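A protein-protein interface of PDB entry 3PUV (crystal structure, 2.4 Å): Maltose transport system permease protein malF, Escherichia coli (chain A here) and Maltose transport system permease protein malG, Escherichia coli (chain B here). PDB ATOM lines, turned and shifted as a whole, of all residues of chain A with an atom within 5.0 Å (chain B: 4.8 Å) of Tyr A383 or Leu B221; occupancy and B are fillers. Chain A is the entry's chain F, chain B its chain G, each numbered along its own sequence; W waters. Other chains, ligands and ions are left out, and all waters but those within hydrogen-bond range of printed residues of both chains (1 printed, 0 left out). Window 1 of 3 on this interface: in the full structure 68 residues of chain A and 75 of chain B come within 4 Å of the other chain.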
ATOM      1  N   TYR A 325       9.568  -3.496  10.434  1.00  0.00           N
ATOM      2  CA  TYR A 325      10.958  -3.865  10.180  1.00  0.00           C
ATOM      3  C   TYR A 325      11.382  -3.453   8.767  1.00  0.00           C
ATOM      4  O   TYR A 325      12.575  -3.401   8.458  1.00  0.00           O
ATOM      5  CB  TYR A 325      11.107  -5.373  10.375  1.00  0.00           C
ATOM      6  CG  TYR A 325      12.516  -5.913  10.532  1.00  0.00           C
ATOM      7  CD1 TYR A 325      13.522  -5.170  11.159  1.00  0.00           C
ATOM      8  CD2 TYR A 325      12.828  -7.200  10.087  1.00  0.00           C
ATOM      9  CE1 TYR A 325      14.812  -5.691  11.306  1.00  0.00           C
ATOM     10  CE2 TYR A 325      14.101  -7.726  10.233  1.00  0.00           C
ATOM     11  CZ  TYR A 325      15.085  -6.974  10.845  1.00  0.00           C
ATOM     12  OH  TYR A 325      16.343  -7.514  10.982  1.00  0.00           O
ATOM     13  N   GLY A 380      11.321  -5.206  17.277  1.00  0.00           N
ATOM     14  CA  GLY A 380      11.964  -6.518  17.234  1.00  0.00           C
ATOM     15  C   GLY A 380      11.137  -7.759  16.945  1.00  0.00           C
ATOM     16  O   GLY A 380      11.707  -8.826  16.693  1.00  0.00           O
ATOM     17  N   TYR A 381       9.809  -7.649  16.979  1.00  0.00           N
ATOM     18  CA  TYR A 381       8.972  -8.833  16.741  1.00  0.00           C
ATOM     19  C   TYR A 381       9.034  -9.396  15.305  1.00  0.00           C
ATOM     20  O   TYR A 381       8.999 -10.617  15.140  1.00  0.00           O
ATOM     21  CB  TYR A 381       7.522  -8.653  17.237  1.00  0.00           C
ATOM     22  CG  TYR A 381       6.584  -7.959  16.276  1.00  0.00           C
ATOM     23  CD1 TYR A 381       5.983  -8.660  15.229  1.00  0.00           C
ATOM     24  CD2 TYR A 381       6.281  -6.611  16.425  1.00  0.00           C
ATOM     25  CE1 TYR A 381       5.121  -8.027  14.341  1.00  0.00           C
ATOM     26  CE2 TYR A 381       5.419  -5.965  15.542  1.00  0.00           C
ATOM     27  CZ  TYR A 381       4.842  -6.680  14.503  1.00  0.00           C
ATOM     28  OH  TYR A 381       3.991  -6.049  13.624  1.00  0.00           O
ATOM     29  N   PRO A 382       9.138  -8.527  14.268  1.00  0.00           N
ATOM     30  CA  PRO A 382       9.157  -9.085  12.913  1.00  0.00           C
ATOM     31  C   PRO A 382      10.382  -9.951  12.630  1.00  0.00           C
ATOM     32  O   PRO A 382      10.282 -10.913  11.869  1.00  0.00           O
ATOM     33  CB  PRO A 382       9.165  -7.842  12.019  1.00  0.00           C
ATOM     34  CG  PRO A 382       8.590  -6.768  12.861  1.00  0.00           C
ATOM     35  CD  PRO A 382       9.130  -7.052  14.227  1.00  0.00           C
ATOM     36  N   TYR A 383      11.515  -9.616  13.244  1.00  0.00           N
ATOM     37  CA  TYR A 383      12.734 -10.414  13.127  1.00  0.00           C
ATOM     38  C   TYR A 383      12.478 -11.854  13.570  1.00  0.00           C
ATOM     39  O   TYR A 383      12.741 -12.801  12.824  1.00  0.00           O
ATOM     40  CB  TYR A 383      13.862  -9.787  13.952  1.00  0.00           C
ATOM     41  CG  TYR A 383      15.131 -10.611  14.029  1.00  0.00           C
ATOM     42  CD1 TYR A 383      15.966 -10.755  12.918  1.00  0.00           C
ATOM     43  CD2 TYR A 383      15.507 -11.238  15.218  1.00  0.00           C
ATOM     44  CE1 TYR A 383      17.134 -11.508  12.985  1.00  0.00           C
ATOM     45  CE2 TYR A 383      16.679 -11.992  15.298  1.00  0.00           C
ATOM     46  CZ  TYR A 383      17.487 -12.120  14.177  1.00  0.00           C
ATOM     47  OH  TYR A 383      18.640 -12.869  14.254  1.00  0.00           O
ATOM     48  N   MET A 384      11.941 -12.000  14.781  1.00  0.00           N
ATOM     49  CA  MET A 384      11.651 -13.307  15.360  1.00  0.00           C
ATOM     50  C   MET A 384      10.528 -14.028  14.628  1.00  0.00           C
ATOM     51  O   MET A 384      10.566 -15.249  14.480  1.00  0.00           O
ATOM     52  CB  MET A 384      11.340 -13.179  16.848  1.00  0.00           C
ATOM     53  CG  MET A 384      12.554 -12.832  17.690  1.00  0.00           C
ATOM     54  SD  MET A 384      13.848 -14.090  17.575  1.00  0.00           S
ATOM     55  CE  MET A 384      15.141 -13.304  18.540  1.00  0.00           C
ATOM     56  N   MET A 385       9.545 -13.263  14.162  1.00  0.00           N
ATOM     57  CA  MET A 385       8.437 -13.804  13.381  1.00  0.00           C
ATOM     58  C   MET A 385       8.903 -14.381  12.041  1.00  0.00           C
ATOM     59  O   MET A 385       8.443 -15.445  11.627  1.00  0.00           O
ATOM     60  CB  MET A 385       7.379 -12.729  13.141  1.00  0.00           C
ATOM     61  CG  MET A 385       6.142 -13.243  12.435  1.00  0.00           C
ATOM     62  SD  MET A 385       5.176 -11.930  11.691  1.00  0.00           S
ATOM     63  CE  MET A 385       3.903 -12.896  10.878  1.00  0.00           C
ATOM     64  N   ILE A 386       9.809 -13.674  11.368  1.00  0.00           N
ATOM     65  CA  ILE A 386      10.346 -14.132  10.088  1.00  0.00           C
ATOM     66  C   ILE A 386      11.150 -15.416  10.288  1.00  0.00           C
ATOM     67  O   ILE A 386      11.038 -16.357   9.498  1.00  0.00           O
ATOM     68  CB  ILE A 386      11.187 -13.032   9.386  1.00  0.00           C
ATOM     69  CG1 ILE A 386      10.271 -11.912   8.877  1.00  0.00           C
ATOM     70  CG2 ILE A 386      11.980 -13.616   8.219  1.00  0.00           C
ATOM     71  CD1 ILE A 386      10.991 -10.617   8.502  1.00  0.00           C
ATOM     72  N   LEU A 387      11.945 -15.450  11.356  1.00  0.00           N
ATOM     73  CA  LEU A 387      12.682 -16.653  11.734  1.00  0.00           C
ATOM     74  C   LEU A 387      11.734 -17.824  11.959  1.00  0.00           C
ATOM     75  O   LEU A 387      11.939 -18.904  11.415  1.00  0.00           O
ATOM     76  CB  LEU A 387      13.531 -16.405  12.984  1.00  0.00           C
ATOM     77  CG  LEU A 387      14.834 -15.626  12.793  1.00  0.00           C
ATOM     78  CD1 LEU A 387      15.365 -15.168  14.136  1.00  0.00           C
ATOM     79  CD2 LEU A 387      15.879 -16.459  12.056  1.00  0.00           C
ATOM     80  N   LEU A 429      19.908 -17.975  18.466  1.00  0.00           N
ATOM     81  CA  LEU A 429      19.352 -16.702  18.014  1.00  0.00           C
ATOM     82  C   LEU A 429      18.876 -15.845  19.179  1.00  0.00           C
ATOM     83  O   LEU A 429      18.953 -14.618  19.125  1.00  0.00           O
ATOM     84  CB  LEU A 429      18.220 -16.935  17.012  1.00  0.00           C
ATOM     85  CG  LEU A 429      18.684 -17.557  15.691  1.00  0.00           C
ATOM     86  CD1 LEU A 429      17.531 -18.201  14.935  1.00  0.00           C
ATOM     87  CD2 LEU A 429      19.411 -16.531  14.824  1.00  0.00           C
ATOM     88  N   LEU B 172      25.534 -15.843  12.322  1.00  0.00           N
ATOM     89  CA  LEU B 172      24.199 -16.210  12.780  1.00  0.00           C
ATOM     90  C   LEU B 172      23.409 -16.991  11.738  1.00  0.00           C
ATOM     91  O   LEU B 172      22.700 -17.938  12.083  1.00  0.00           O
ATOM     92  CB  LEU B 172      23.417 -14.972  13.222  1.00  0.00           C
ATOM     93  CG  LEU B 172      23.554 -14.603  14.697  1.00  0.00           C
ATOM     94  CD1 LEU B 172      22.822 -13.309  14.966  1.00  0.00           C
ATOM     95  CD2 LEU B 172      23.013 -15.726  15.576  1.00  0.00           C
ATOM     96  N   HIS B 173      23.532 -16.589  10.473  1.00  0.00           N
ATOM     97  CA  HIS B 173      22.853 -17.273   9.374  1.00  0.00           C
ATOM     98  C   HIS B 173      23.348 -18.712   9.222  1.00  0.00           C
ATOM     99  O   HIS B 173      22.567 -19.610   8.909  1.00  0.00           O
ATOM    100  CB  HIS B 173      23.006 -16.500   8.064  1.00  0.00           C
ATOM    101  CG  HIS B 173      22.402 -15.129   8.095  1.00  0.00           C
ATOM    102  ND1 HIS B 173      21.084 -14.903   8.433  1.00  0.00           N
ATOM    103  CD2 HIS B 173      22.930 -13.915   7.811  1.00  0.00           C
ATOM    104  CE1 HIS B 173      20.831 -13.607   8.368  1.00  0.00           C
ATOM    105  NE2 HIS B 173      21.934 -12.986   7.992  1.00  0.00           N
ATOM    106  N   VAL B 217      14.207 -17.312   4.427  1.00  0.00           N
ATOM    107  CA  VAL B 217      14.394 -16.567   5.677  1.00  0.00           C
ATOM    108  C   VAL B 217      15.729 -15.822   5.696  1.00  0.00           C
ATOM    109  O   VAL B 217      15.764 -14.614   5.953  1.00  0.00           O
ATOM    110  CB  VAL B 217      14.266 -17.483   6.919  1.00  0.00           C
ATOM    111  CG1 VAL B 217      14.801 -16.799   8.184  1.00  0.00           C
ATOM    112  CG2 VAL B 217      12.823 -17.902   7.111  1.00  0.00           C
ATOM    113  N   VAL B 218      16.817 -16.532   5.400  1.00  0.00           N
ATOM    114  CA  VAL B 218      18.139 -15.914   5.393  1.00  0.00           C
ATOM    115  C   VAL B 218      18.249 -14.828   4.315  1.00  0.00           C
ATOM    116  O   VAL B 218      18.839 -13.773   4.566  1.00  0.00           O
ATOM    117  CB  VAL B 218      19.283 -16.956   5.280  1.00  0.00           C
ATOM    118  CG1 VAL B 218      20.638 -16.267   5.114  1.00  0.00           C
ATOM    119  CG2 VAL B 218      19.309 -17.846   6.510  1.00  0.00           C
ATOM    120  N   PHE B 219      17.662 -15.071   3.140  1.00  0.00           N
ATOM    121  CA  PHE B 219      17.637 -14.062   2.075  1.00  0.00           C
ATOM    122  C   PHE B 219      16.895 -12.804   2.519  1.00  0.00           C
ATOM    123  O   PHE B 219      17.388 -11.686   2.334  1.00  0.00           O
ATOM    124  CB  PHE B 219      17.012 -14.606   0.785  1.00  0.00           C
ATOM    125  CG  PHE B 219      17.125 -13.662  -0.383  1.00  0.00           C
ATOM    126  CD1 PHE B 219      18.229 -13.712  -1.229  1.00  0.00           C
ATOM    127  CD2 PHE B 219      16.142 -12.710  -0.629  1.00  0.00           C
ATOM    128  CE1 PHE B 219      18.348 -12.837  -2.306  1.00  0.00           C
ATOM    129  CE2 PHE B 219      16.255 -11.826  -1.699  1.00  0.00           C
ATOM    130  CZ  PHE B 219      17.359 -11.889  -2.538  1.00  0.00           C
ATOM    131  N   ILE B 220      15.709 -12.997   3.094  1.00  0.00           N
ATOM    132  CA  ILE B 220      14.893 -11.898   3.597  1.00  0.00           C
ATOM    133  C   ILE B 220      15.649 -11.091   4.648  1.00  0.00           C
ATOM    134  O   ILE B 220      15.777  -9.869   4.519  1.00  0.00           O
ATOM    135  CB  ILE B 220      13.554 -12.403   4.181  1.00  0.00           C
ATOM    136  CG1 ILE B 220      12.622 -12.862   3.056  1.00  0.00           C
ATOM    137  CG2 ILE B 220      12.886 -11.318   5.043  1.00  0.00           C
ATOM    138  CD1 ILE B 220      11.523 -13.796   3.526  1.00  0.00           C
ATOM    139  N   LEU B 221      16.166 -11.777   5.668  1.00  0.00           N
ATOM    140  CA  LEU B 221      16.871 -11.103   6.757  1.00  0.00           C
ATOM    141  C   LEU B 221      18.087 -10.312   6.288  1.00  0.00           C
ATOM    142  O   LEU B 221      18.408  -9.271   6.865  1.00  0.00           O
ATOM    143  CB  LEU B 221      17.260 -12.086   7.857  1.00  0.00           C
ATOM    144  CG  LEU B 221      16.099 -12.612   8.707  1.00  0.00           C
ATOM    145  CD1 LEU B 221      16.584 -13.696   9.646  1.00  0.00           C
ATOM    146  CD2 LEU B 221      15.415 -11.498   9.485  1.00  0.00           C
ATOM    147  N   SER B 222      18.738 -10.799   5.233  1.00  0.00           N
ATOM    148  CA  SER B 222      19.890 -10.125   4.641  1.00  0.00           C
ATOM    149  C   SER B 222      19.505  -8.947   3.759  1.00  0.00           C
ATOM    150  O   SER B 222      20.198  -7.929   3.745  1.00  0.00           O
ATOM    151  CB  SER B 222      20.722 -11.108   3.826  1.00  0.00           C
ATOM    152  OG  SER B 222      21.310 -12.060   4.681  1.00  0.00           O
ATOM    153  N   PHE B 223      18.414  -9.098   3.011  1.00  0.00           N
ATOM    154  CA  PHE B 223      17.936  -8.040   2.131  1.00  0.00           C
ATOM    155  C   PHE B 223      17.505  -6.816   2.941  1.00  0.00           C
ATOM    156  O   PHE B 223      17.830  -5.696   2.579  1.00  0.00           O
ATOM    157  CB  PHE B 223      16.793  -8.543   1.246  1.00  0.00           C
ATOM    158  CG  PHE B 223      16.455  -7.621   0.115  1.00  0.00           C
ATOM    159  CD1 PHE B 223      17.164  -7.679  -1.080  1.00  0.00           C
ATOM    160  CD2 PHE B 223      15.432  -6.689   0.243  1.00  0.00           C
ATOM    161  CE1 PHE B 223      16.857  -6.828  -2.134  1.00  0.00           C
ATOM    162  CE2 PHE B 223      15.115  -5.834  -0.803  1.00  0.00           C
ATOM    163  CZ  PHE B 223      15.831  -5.901  -1.995  1.00  0.00           C
ATOM    164  N   ILE B 224      16.780  -7.046   4.036  1.00  0.00           N
ATOM    165  CA  ILE B 224      16.396  -5.986   4.976  1.00  0.00           C
ATOM    166  C   ILE B 224      17.634  -5.313   5.574  1.00  0.00           C
ATOM    167  O   ILE B 224      17.765  -4.081   5.541  1.00  0.00           O
ATOM    168  CB  ILE B 224      15.505  -6.538   6.107  1.00  0.00           C
ATOM    169  CG1 ILE B 224      14.192  -7.075   5.531  1.00  0.00           C
ATOM    170  CG2 ILE B 224      15.255  -5.477   7.173  1.00  0.00           C
ATOM    171  CD1 ILE B 224      13.365  -7.885   6.511  1.00  0.00           C
ATOM    172  N   ALA B 225      18.540  -6.137   6.100  1.00  0.00           N
ATOM    173  CA  ALA B 225      19.789  -5.670   6.682  1.00  0.00           C
ATOM    174  C   ALA B 225      20.518  -4.706   5.741  1.00  0.00           C
ATOM    175  O   ALA B 225      20.947  -3.627   6.158  1.00  0.00           O
ATOM    176  CB  ALA B 225      20.677  -6.853   7.035  1.00  0.00           C
HETATM  177  O   HOH W   1      18.903  -9.158   9.760  1.00  0.00           O
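Water W1 bridges the backbone carbonyl oxygen of Leu B221 (2.9 Å) and the side-chain hydroxyl of Tyr A325 (3.3 Å).
Among the printed residues, merely in contact across the chains: Ile A386 with Val B217 (3.4 Å), Tyr A383 with Leu B221 (3.6 Å), Tyr A325 with Ile B224 (3.6 Å), Leu A387 with Leu B221 (3.7 Å) and Leu A429 with Leu B172 (3.8 Å).
Of the printed residues of chain B, Tyr A325 touches Ile B224 (3.6 Å).
Of the printed residues of chain B, Tyr A383 touches Leu B221 (3.6 Å).
Met A385 touches none of the printed residues of chain B.
Of the printed residues of chain B, Leu A387 touches Leu B221.
Of the printed residues of chain A, Val B217 touches Ile A386 (3.4 Å).
Leu B221 touches just these residues of chain A: Tyr A383 and Leu A387.
The nearest residue of chain A that does not touch Leu B221 is Tyr A325 (4.1 Å).
The nearest printed residue of chain B that does not touch Ile A386 is Ile B220 (4.01 Å).
Of the 10 printed residues of chain A, 5 touch a printed residue of chain B.
Hydrophobic or aromatic side chains of chain A within 4 Å of the printed part of chain B: Tyr A325, Tyr A383, Leu A387 and Leu A429.
Along chain A the printed residues that touch a printed residue of chain B span positions 325 to 429.
Hydrophobic or aromatic side chains of chain B within 4 Å of the printed part of chain A: Leu B172, Val B217, Leu B221 and Ile B224.
Among the printed residues, 5 pairs touch across the chains.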
